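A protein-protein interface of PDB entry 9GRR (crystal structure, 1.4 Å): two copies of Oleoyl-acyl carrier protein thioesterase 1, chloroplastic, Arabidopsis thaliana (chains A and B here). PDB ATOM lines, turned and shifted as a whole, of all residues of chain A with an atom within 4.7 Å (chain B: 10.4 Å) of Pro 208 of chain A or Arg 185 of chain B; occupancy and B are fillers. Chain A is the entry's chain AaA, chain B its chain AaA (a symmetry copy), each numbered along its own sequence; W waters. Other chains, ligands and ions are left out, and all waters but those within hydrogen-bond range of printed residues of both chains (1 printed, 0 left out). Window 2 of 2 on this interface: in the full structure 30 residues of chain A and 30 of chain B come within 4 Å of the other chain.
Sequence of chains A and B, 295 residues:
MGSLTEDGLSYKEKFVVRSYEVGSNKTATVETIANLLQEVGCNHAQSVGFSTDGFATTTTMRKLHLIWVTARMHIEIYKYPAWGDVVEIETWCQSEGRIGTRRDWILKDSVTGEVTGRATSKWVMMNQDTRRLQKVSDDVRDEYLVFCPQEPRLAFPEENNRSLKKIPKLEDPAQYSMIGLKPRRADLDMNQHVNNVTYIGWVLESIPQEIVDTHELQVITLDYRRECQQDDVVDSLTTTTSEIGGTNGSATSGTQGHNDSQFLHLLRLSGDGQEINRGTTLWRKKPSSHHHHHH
No position is printed for both chains.
Arg 185 of chain B touches just these residues of chain A: Leu 204, Glu 205, Ile 207, Pro 208, Gln 209 and Val 212. Of chain B, only Arg 185 (2.8 Å) comes within 4 Å of Ile 207 of chain A. No residue of chain B comes within 4 Å of Ile 211 of chain A. Of the printed residues of chain A, Arg 184 of chain B touches Glu 205. Of the printed residues of chain B, Gln 209 of chain A touches Arg 185 (2.9 Å) and Gln 192 (3.997 Å). Pro 183 of chain B touches none of the printed residues of chain A. The nearest residue of chain B that does not touch Pro 208 of chain A is Gln 192 of chain B (9.7 Å).
Among the printed residues, pairs that only touch across the chains: Glu 205 of chain A with Arg 184 of chain B (3.4 Å), Val 212 of chain A with Arg 185 of chain B (3.6 Å), Pro 208 of chain A with Arg 185 of chain B (3.9 Å) and Gln 209 of chain A with Gln 192 of chain B (3.997 Å).
OD2 of Asp 187 of chain B sits at hydrogen-bond distance from N of Arg 184 of chain B, at 2.9 Å. The backbone NH (N) of Gln 192 of chain B sits at hydrogen-bond distance from the side-chain carboxylate (OD1) of Asp 189 of chain B (3.1 Å). O of Gln 192 of chain B is in hydrogen-bond range of NE2 of Gln 230 of chain B, at 3.0 Å.
Hydrophobic or aromatic side chains of chain A that line the printed part of chain B: Val 212. Of the 19 printed residues of chain B, 3 touch a printed residue of chain A. Among the printed residues, 8 pairs touch across the chains. Among the printed residues, no Asp or Glu carboxylate lies within 4 Å of a Lys or Arg side-chain nitrogen of the other chain.
O of Leu 204 of chain A lies within hydrogen-bond range of NH1 of Arg 185 of chain B, 2.8 Å away. The side-chain carboxylate (OE1) of Glu 205 of chain A sits at hydrogen-bond distance from the backbone NH (N) of Arg 185 of chain B. O of Ile 207 of chain A sits at hydrogen-bond distance from NH2 of Arg 185 of chain B (2.8 Å). The guanidinium group (NE) of Arg 185 of chain B sits at hydrogen-bond distance from the side-chain amide oxygen (OE1) of Gln 209 of chain A (2.9 Å).
Water W1 lies within hydrogen-bond range of the side-chain carboxylate (OE2) of Glu 205 of chain A (2.8 Å) and the backbone carbonyl oxygen (O) of Pro 183 of chain B (2.9 Å).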
ATOM      1  N   TYR A 176       1.627  22.939   4.752  1.00  0.00           N
ATOM      2  CA  TYR A 176       2.749  22.400   5.543  1.00  0.00           C
ATOM      3  C   TYR A 176       3.249  23.477   6.490  1.00  0.00           C
ATOM      4  O   TYR A 176       3.161  24.674   6.165  1.00  0.00           O
ATOM      5  CB  TYR A 176       3.877  21.945   4.621  1.00  0.00           C
ATOM      6  CG  TYR A 176       3.467  20.979   3.545  1.00  0.00           C
ATOM      7  CD1 TYR A 176       2.994  19.708   3.860  1.00  0.00           C
ATOM      8  CD2 TYR A 176       3.578  21.319   2.206  1.00  0.00           C
ATOM      9  CE1 TYR A 176       2.622  18.819   2.865  1.00  0.00           C
ATOM     10  CE2 TYR A 176       3.225  20.436   1.198  1.00  0.00           C
ATOM     11  CZ  TYR A 176       2.736  19.183   1.532  1.00  0.00           C
ATOM     12  OH  TYR A 176       2.396  18.299   0.548  1.00  0.00           O
ATOM     13  N   LEU A 204      12.947  26.127   3.909  1.00  0.00           N
ATOM     14  CA  LEU A 204      13.052  24.740   3.390  1.00  0.00           C
ATOM     15  C   LEU A 204      12.562  23.742   4.446  1.00  0.00           C
ATOM     16  O   LEU A 204      12.113  22.636   4.060  1.00  0.00           O
ATOM     17  CB  LEU A 204      14.484  24.417   2.940  1.00  0.00           C
ATOM     18  CG  LEU A 204      15.065  25.248   1.787  1.00  0.00           C
ATOM     19  CD1 LEU A 204      16.170  24.462   1.097  1.00  0.00           C
ATOM     20  CD2 LEU A 204      14.031  25.684   0.762  1.00  0.00           C
ATOM     21  N   GLU A 205      12.620  24.095   5.731  1.00  0.00           N
ATOM     22  CA  GLU A 205      12.239  23.145   6.814  1.00  0.00           C
ATOM     23  C   GLU A 205      10.790  22.697   6.674  1.00  0.00           C
ATOM     24  O   GLU A 205      10.478  21.583   7.132  1.00  0.00           O
ATOM     25  CB  GLU A 205      12.379  23.765   8.195  1.00  0.00           C
ATOM     26  CG  GLU A 205      13.776  23.643   8.744  1.00  0.00           C
ATOM     27  CD  GLU A 205      14.191  22.188   8.907  1.00  0.00           C
ATOM     28  OE1 GLU A 205      15.011  21.711   8.100  1.00  0.00           O
ATOM     29  OE2 GLU A 205      13.664  21.518   9.823  1.00  0.00           O
ATOM     30  N   SER A 206       9.918  23.528   6.123  1.00  0.00           N
ATOM     31  CA  SER A 206       8.486  23.167   5.983  1.00  0.00           C
ATOM     32  C   SER A 206       8.210  22.446   4.668  1.00  0.00           C
ATOM     33  O   SER A 206       7.037  22.104   4.448  1.00  0.00           O
ATOM     34  CB  SER A 206       7.583  24.362   6.157  1.00  0.00           C
ATOM     35  OG  SER A 206       7.901  25.389   5.241  1.00  0.00           O
ATOM     36  N   ILE A 207       9.214  22.259   3.798  1.00  0.00           N
ATOM     37  CA  ILE A 207       9.019  21.466   2.553  1.00  0.00           C
ATOM     38  C   ILE A 207       9.014  20.002   2.977  1.00  0.00           C
ATOM     39  O   ILE A 207       9.904  19.593   3.702  1.00  0.00           O
ATOM     40  CB  ILE A 207      10.111  21.762   1.512  1.00  0.00           C
ATOM     41  CG1 ILE A 207      10.076  23.231   1.085  1.00  0.00           C
ATOM     42  CG2 ILE A 207      10.040  20.787   0.339  1.00  0.00           C
ATOM     43  CD1 ILE A 207       9.987  23.473  -0.388  1.00  0.00           C
ATOM     44  N   PRO A 208       8.038  19.183   2.528  1.00  0.00           N
ATOM     45  CA  PRO A 208       8.040  17.764   2.896  1.00  0.00           C
ATOM     46  C   PRO A 208       9.328  17.023   2.519  1.00  0.00           C
ATOM     47  O   PRO A 208       9.917  17.280   1.480  1.00  0.00           O
ATOM     48  CB  PRO A 208       6.854  17.157   2.140  1.00  0.00           C
ATOM     49  CG  PRO A 208       5.967  18.341   1.789  1.00  0.00           C
ATOM     50  CD  PRO A 208       6.858  19.569   1.740  1.00  0.00           C
ATOM     51  N   GLN A 209       9.731  16.084   3.377  1.00  0.00           N
ATOM     52  CA  GLN A 209      10.972  15.289   3.197  1.00  0.00           C
ATOM     53  C   GLN A 209      10.931  14.554   1.847  1.00  0.00           C
ATOM     54  O   GLN A 209      11.987  14.455   1.203  1.00  0.00           O
ATOM     55  CB  GLN A 209      11.152  14.316   4.364  1.00  0.00           C
ATOM     56  CG  GLN A 209      12.518  13.647   4.389  1.00  0.00           C
ATOM     57  CD  GLN A 209      13.641  14.634   4.584  1.00  0.00           C
ATOM     58  OE1 GLN A 209      13.677  15.378   5.563  1.00  0.00           O
ATOM     59  NE2 GLN A 209      14.568  14.659   3.638  1.00  0.00           N
ATOM     60  N   GLU A 210       9.757  14.056   1.448  1.00  0.00           N
ATOM     61  CA  GLU A 210       9.565  13.322   0.166  1.00  0.00           C
ATOM     62  C   GLU A 210       9.969  14.224  -1.001  1.00  0.00           C
ATOM     63  O   GLU A 210      10.602  13.708  -1.934  1.00  0.00           O
ATOM     64  CB  GLU A 210       8.118  12.873  -0.065  1.00  0.00           C
ATOM     65  CG  GLU A 210       7.589  11.894   0.965  1.00  0.00           C
ATOM     66  CD  GLU A 210       6.993  12.515   2.215  1.00  0.00           C
ATOM     67  OE1 GLU A 210       6.738  11.756   3.178  1.00  0.00           O
ATOM     68  OE2 GLU A 210       6.792  13.751   2.230  1.00  0.00           O
ATOM     69  N   ILE A 211       9.605  15.515  -0.961  1.00  0.00           N
ATOM     70  CA  ILE A 211       9.958  16.469  -2.061  1.00  0.00           C
ATOM     71  C   ILE A 211      11.473  16.657  -2.035  1.00  0.00           C
ATOM     72  O   ILE A 211      12.100  16.545  -3.111  1.00  0.00           O
ATOM     73  CB  ILE A 211       9.229  17.831  -1.987  1.00  0.00           C
ATOM     74  CG1 ILE A 211       7.779  17.729  -2.454  1.00  0.00           C
ATOM     75  CG2 ILE A 211       9.972  18.861  -2.825  1.00  0.00           C
ATOM     76  CD1 ILE A 211       6.863  16.948  -1.551  1.00  0.00           C
ATOM     77  N   VAL A 212      12.061  16.923  -0.863  1.00  0.00           N
ATOM     78  CA  VAL A 212      13.539  17.124  -0.759  1.00  0.00           C
ATOM     79  C   VAL A 212      14.264  15.859  -1.234  1.00  0.00           C
ATOM     80  O   VAL A 212      15.288  15.990  -1.906  1.00  0.00           O
ATOM     81  CB  VAL A 212      13.971  17.547   0.663  1.00  0.00           C
ATOM     82  CG1 VAL A 212      15.485  17.571   0.818  1.00  0.00           C
ATOM     83  CG2 VAL A 212      13.389  18.902   1.017  1.00  0.00           C
ATOM     84  N   LYS B 182      16.023  20.699  18.366  1.00  0.00           N
ATOM     85  CA  LYS B 182      15.793  19.819  17.208  1.00  0.00           C
ATOM     86  C   LYS B 182      16.776  20.210  16.119  1.00  0.00           C
ATOM     87  O   LYS B 182      16.987  21.391  15.856  1.00  0.00           O
ATOM     88  CB  LYS B 182      14.377  19.958  16.646  1.00  0.00           C
ATOM     89  CG  LYS B 182      13.228  19.723  17.613  1.00  0.00           C
ATOM     90  CD  LYS B 182      11.926  20.307  17.094  1.00  0.00           C
ATOM     91  CE  LYS B 182      11.431  19.601  15.845  1.00  0.00           C
ATOM     92  NZ  LYS B 182      10.120  20.127  15.392  1.00  0.00           N
ATOM     93  N   PRO B 183      17.361  19.203  15.457  1.00  0.00           N
ATOM     94  CA  PRO B 183      18.172  19.420  14.271  1.00  0.00           C
ATOM     95  C   PRO B 183      17.280  19.897  13.113  1.00  0.00           C
ATOM     96  O   PRO B 183      16.088  19.590  13.073  1.00  0.00           O
ATOM     97  CB  PRO B 183      18.849  18.056  14.032  1.00  0.00           C
ATOM     98  CG  PRO B 183      17.953  17.050  14.703  1.00  0.00           C
ATOM     99  CD  PRO B 183      17.273  17.790  15.832  1.00  0.00           C
ATOM    100  N   ARG B 184      17.860  20.709  12.226  1.00  0.00           N
ATOM    101  CA  ARG B 184      17.242  21.031  10.928  1.00  0.00           C
ATOM    102  C   ARG B 184      18.088  20.319   9.874  1.00  0.00           C
ATOM    103  O   ARG B 184      19.077  19.669  10.230  1.00  0.00           O
ATOM    104  CB  ARG B 184      17.059  22.539  10.705  1.00  0.00           C
ATOM    105  CG  ARG B 184      18.287  23.413  10.903  1.00  0.00           C
ATOM    106  CD  ARG B 184      17.871  24.863  10.737  1.00  0.00           C
ATOM    107  NE  ARG B 184      18.948  25.828  10.857  1.00  0.00           N
ATOM    108  CZ  ARG B 184      19.621  26.344   9.836  1.00  0.00           C
ATOM    109  NH1 ARG B 184      19.361  25.967   8.593  1.00  0.00           N
ATOM    110  NH2 ARG B 184      20.564  27.232  10.077  1.00  0.00           N
ATOM    111  N   ARG B 185      17.651  20.357   8.624  1.00  0.00           N
ATOM    112  CA  ARG B 185      18.307  19.552   7.566  1.00  0.00           C
ATOM    113  C   ARG B 185      19.772  19.970   7.460  1.00  0.00           C
ATOM    114  O   ARG B 185      20.604  19.093   7.165  1.00  0.00           O
ATOM    115  CB  ARG B 185      17.520  19.662   6.264  1.00  0.00           C
ATOM    116  CG  ARG B 185      16.192  18.926   6.345  1.00  0.00           C
ATOM    117  CD  ARG B 185      15.485  18.837   5.017  1.00  0.00           C
ATOM    118  NE  ARG B 185      14.169  18.255   5.231  1.00  0.00           N
ATOM    119  CZ  ARG B 185      13.009  18.831   4.926  1.00  0.00           C
ATOM    120  NH1 ARG B 185      12.967  20.030   4.372  1.00  0.00           N
ATOM    121  NH2 ARG B 185      11.881  18.189   5.172  1.00  0.00           N
ATOM    122  N   ALA B 186      20.107  21.237   7.710  1.00  0.00           N
ATOM    123  CA  ALA B 186      21.511  21.716   7.629  1.00  0.00           C
ATOM    124  C   ALA B 186      22.403  20.958   8.630  1.00  0.00           C
ATOM    125  O   ALA B 186      23.625  20.910   8.420  1.00  0.00           O
ATOM    126  CB  ALA B 186      21.592  23.213   7.814  1.00  0.00           C
ATOM    127  N   ASP B 187      21.833  20.365   9.679  1.00  0.00           N
ATOM    128  CA  ASP B 187      22.615  19.635  10.714  1.00  0.00           C
ATOM    129  C   ASP B 187      22.932  18.197  10.289  1.00  0.00           C
ATOM    130  O   ASP B 187      23.651  17.531  11.032  1.00  0.00           O
ATOM    131  CB  ASP B 187      21.884  19.616  12.063  1.00  0.00           C
ATOM    132  CG  ASP B 187      21.693  21.002  12.660  1.00  0.00           C
ATOM    133  OD1 ASP B 187      22.685  21.731  12.743  1.00  0.00           O
ATOM    134  OD2 ASP B 187      20.537  21.391  12.974  1.00  0.00           O
ATOM    135  N   LEU B 188      22.375  17.719   9.173  1.00  0.00           N
ATOM    136  CA  LEU B 188      22.624  16.338   8.699  1.00  0.00           C
ATOM    137  C   LEU B 188      23.785  16.327   7.707  1.00  0.00           C
ATOM    138  O   LEU B 188      23.928  17.283   6.890  1.00  0.00           O
ATOM    139  CB  LEU B 188      21.365  15.761   8.052  1.00  0.00           C
ATOM    140  CG  LEU B 188      20.080  15.886   8.860  1.00  0.00           C
ATOM    141  CD1 LEU B 188      18.920  15.268   8.099  1.00  0.00           C
ATOM    142  CD2 LEU B 188      20.236  15.241  10.226  1.00  0.00           C
ATOM    143  N   ASP B 189      24.573  15.266   7.767  1.00  0.00           N
ATOM    144  CA  ASP B 189      25.709  15.086   6.838  1.00  0.00           C
ATOM    145  C   ASP B 189      25.233  14.386   5.566  1.00  0.00           C
ATOM    146  O   ASP B 189      24.015  14.167   5.391  1.00  0.00           O
ATOM    147  CB  ASP B 189      26.852  14.338   7.503  1.00  0.00           C
ATOM    148  CG  ASP B 189      26.512  12.899   7.846  1.00  0.00           C
ATOM    149  OD1 ASP B 189      25.520  12.364   7.307  1.00  0.00           O
ATOM    150  OD2 ASP B 189      27.226  12.350   8.672  1.00  0.00           O
ATOM    151  N   MET B 190      26.170  14.063   4.684  1.00  0.00           N
ATOM    152  CA  MET B 190      25.826  13.512   3.350  1.00  0.00           C
ATOM    153  C   MET B 190      25.174  12.126   3.498  1.00  0.00           C
ATOM    154  O   MET B 190      24.499  11.684   2.543  1.00  0.00           O
ATOM    155  CB  MET B 190      27.061  13.469   2.446  1.00  0.00           C
ATOM    156  CG  MET B 190      28.110  12.451   2.849  1.00  0.00           C
ATOM    157  SD  MET B 190      29.523  12.505   1.708  1.00  0.00           S
ATOM    158  CE  MET B 190      30.389  13.961   2.295  1.00  0.00           C
ATOM    159  N   ASN B 191      25.246  11.522   4.692  1.00  0.00           N
ATOM    160  CA  ASN B 191      24.636  10.197   4.999  1.00  0.00           C
ATOM    161  C   ASN B 191      23.328  10.369   5.785  1.00  0.00           C
ATOM    162  O   ASN B 191      22.775   9.353   6.247  1.00  0.00           O
ATOM    163  CB  ASN B 191      25.645   9.310   5.727  1.00  0.00           C
ATOM    164  CG  ASN B 191      26.983   9.262   5.012  1.00  0.00           C
ATOM    165  OD1 ASN B 191      27.062   8.902   3.838  1.00  0.00           O
ATOM    166  ND2 ASN B 191      28.047   9.637   5.705  1.00  0.00           N
ATOM    167  N   GLN B 192      22.821  11.601   5.897  1.00  0.00           N
ATOM    168  CA  GLN B 192      21.551  11.938   6.605  1.00  0.00           C
ATOM    169  C   GLN B 192      21.649  11.535   8.079  1.00  0.00           C
ATOM    170  O   GLN B 192      20.596  11.350   8.711  1.00  0.00           O
ATOM    171  CB  GLN B 192      20.336  11.275   5.949  1.00  0.00           C
ATOM    172  CG  GLN B 192      19.993  11.873   4.597  1.00  0.00           C
ATOM    173  CD  GLN B 192      18.551  11.630   4.221  1.00  0.00           C
ATOM    174  OE1 GLN B 192      17.642  12.324   4.676  1.00  0.00           O
ATOM    175  NE2 GLN B 192      18.335  10.633   3.378  1.00  0.00           N
ATOM    176  N   HIS B 193      22.869  11.454   8.607  1.00  0.00           N
ATOM    177  CA  HIS B 193      23.142  11.430  10.062  1.00  0.00           C
ATOM    178  C   HIS B 193      23.344  12.862  10.558  1.00  0.00           C
ATOM    179  O   HIS B 193      23.912  13.701   9.817  1.00  0.00           O
ATOM    180  CB  HIS B 193      24.364  10.561  10.364  1.00  0.00           C
ATOM    181  CG  HIS B 193      24.075   9.108  10.179  1.00  0.00           C
ATOM    182  ND1 HIS B 193      23.940   8.238  11.244  1.00  0.00           N
ATOM    183  CD2 HIS B 193      23.883   8.374   9.062  1.00  0.00           C
ATOM    184  CE1 HIS B 193      23.676   7.029  10.785  1.00  0.00           C
ATOM    185  NE2 HIS B 193      23.633   7.087   9.447  1.00  0.00           N
ATOM    186  N   VAL B 194      22.919  13.114  11.791  1.00  0.00           N
ATOM    187  CA  VAL B 194      23.228  14.382  12.503  1.00  0.00           C
ATOM    188  C   VAL B 194      24.748  14.531  12.565  1.00  0.00           C
ATOM    189  O   VAL B 194      25.435  13.656  13.069  1.00  0.00           O
ATOM    190  CB  VAL B 194      22.573  14.443  13.888  1.00  0.00           C
ATOM    191  CG1 VAL B 194      23.157  15.615  14.673  1.00  0.00           C
ATOM    192  CG2 VAL B 194      21.074  14.619  13.720  1.00  0.00           C
ATOM    193  N   ASN B 195      25.246  15.641  12.035  1.00  0.00           N
ATOM    194  CA  ASN B 195      26.684  15.999  12.078  1.00  0.00           C
ATOM    195  C   ASN B 195      27.163  16.014  13.525  1.00  0.00           C
ATOM    196  O   ASN B 195      26.473  16.635  14.375  1.00  0.00           O
ATOM    197  CB  ASN B 195      26.863  17.386  11.471  1.00  0.00           C
ATOM    198  CG  ASN B 195      28.300  17.795  11.234  1.00  0.00           C
ATOM    199  OD1 ASN B 195      29.184  17.569  12.066  1.00  0.00           O
ATOM    200  ND2 ASN B 195      28.530  18.430  10.096  1.00  0.00           N
ATOM    201  N   THR B 198      27.266  19.305  15.587  1.00  0.00           N
ATOM    202  CA  THR B 198      25.954  19.703  16.110  1.00  0.00           C
ATOM    203  C   THR B 198      25.967  19.494  17.626  1.00  0.00           C
ATOM    204  O   THR B 198      25.427  20.335  18.323  1.00  0.00           O
ATOM    205  CB  THR B 198      24.819  18.914  15.442  1.00  0.00           C
ATOM    206  OG1 THR B 198      25.112  18.966  14.039  1.00  0.00           O
ATOM    207  CG2 THR B 198      23.446  19.463  15.763  1.00  0.00           C
ATOM    208  N   TRP B 202      25.057  22.082  20.552  1.00  0.00           N
ATOM    209  CA  TRP B 202      23.972  21.805  21.532  1.00  0.00           C
ATOM    210  C   TRP B 202      24.484  21.916  22.974  1.00  0.00           C
ATOM    211  O   TRP B 202      23.760  22.446  23.849  1.00  0.00           O
ATOM    212  CB  TRP B 202      23.392  20.438  21.193  1.00  0.00           C
ATOM    213  CG  TRP B 202      22.463  20.499  20.015  1.00  0.00           C
ATOM    214  CD1 TRP B 202      21.834  21.593  19.489  1.00  0.00           C
ATOM    215  CD2 TRP B 202      21.956  19.371  19.292  1.00  0.00           C
ATOM    216  NE1 TRP B 202      20.999  21.234  18.458  1.00  0.00           N
ATOM    217  CE2 TRP B 202      21.075  19.875  18.307  1.00  0.00           C
ATOM    218  CE3 TRP B 202      22.225  18.008  19.346  1.00  0.00           C
ATOM    219  CZ2 TRP B 202      20.408  19.030  17.421  1.00  0.00           C
ATOM    220  CZ3 TRP B 202      21.568  17.172  18.461  1.00  0.00           C
ATOM    221  CH2 TRP B 202      20.698  17.688  17.502  1.00  0.00           C
ATOM    222  N   GLN B 229      19.242  11.033  16.389  1.00  0.00           N
ATOM    223  CA  GLN B 229      18.457  10.916  15.089  1.00  0.00           C
ATOM    224  C   GLN B 229      17.665  12.174  14.639  1.00  0.00           C
ATOM    225  O   GLN B 229      17.426  13.103  15.435  1.00  0.00           O
ATOM    226  CB  GLN B 229      17.375   9.818  15.103  1.00  0.00           C
ATOM    227  CG  GLN B 229      17.730   8.535  15.843  1.00  0.00           C
ATOM    228  CD  GLN B 229      18.897   7.798  15.237  1.00  0.00           C
ATOM    229  OE1 GLN B 229      19.218   7.962  14.063  1.00  0.00           O
ATOM    230  NE2 GLN B 229      19.525   6.952  16.036  1.00  0.00           N
ATOM    231  N   GLN B 230      17.170  12.164  13.385  1.00  0.00           N
ATOM    232  CA  GLN B 230      16.603  13.363  12.690  1.00  0.00           C
ATOM    233  C   GLN B 230      15.287  13.800  13.341  1.00  0.00           C
ATOM    234  O   GLN B 230      15.015  15.021  13.377  1.00  0.00           O
ATOM    235  CB  GLN B 230      16.316  13.104  11.202  1.00  0.00           C
ATOM    236  CG  GLN B 230      17.392  12.318  10.461  1.00  0.00           C
ATOM    237  CD  GLN B 230      16.988  11.995   9.041  1.00  0.00           C
ATOM    238  OE1 GLN B 230      16.126  12.651   8.451  1.00  0.00           O
ATOM    239  NE2 GLN B 230      17.605  10.962   8.488  1.00  0.00           N
ATOM    240  N   ASP B 231      14.505  12.826  13.810  1.00  0.00           N
ATOM    241  CA  ASP B 231      13.105  12.992  14.295  1.00  0.00           C
ATOM    242  C   ASP B 231      13.117  13.307  15.796  1.00  0.00           C
ATOM    243  O   ASP B 231      12.033  13.578  16.365  1.00  0.00           O
ATOM    244  CB  ASP B 231      12.297  11.723  14.001  1.00  0.00           C
ATOM    245  CG  ASP B 231      13.069  10.437  14.263  1.00  0.00           C
ATOM    246  OD1 ASP B 231      13.530  10.254  15.407  1.00  0.00           O
ATOM    247  OD2 ASP B 231      13.238   9.643  13.311  1.00  0.00           O
HETATM  248  O   HOH W   1      14.107  21.720  12.630  1.00  0.00           O
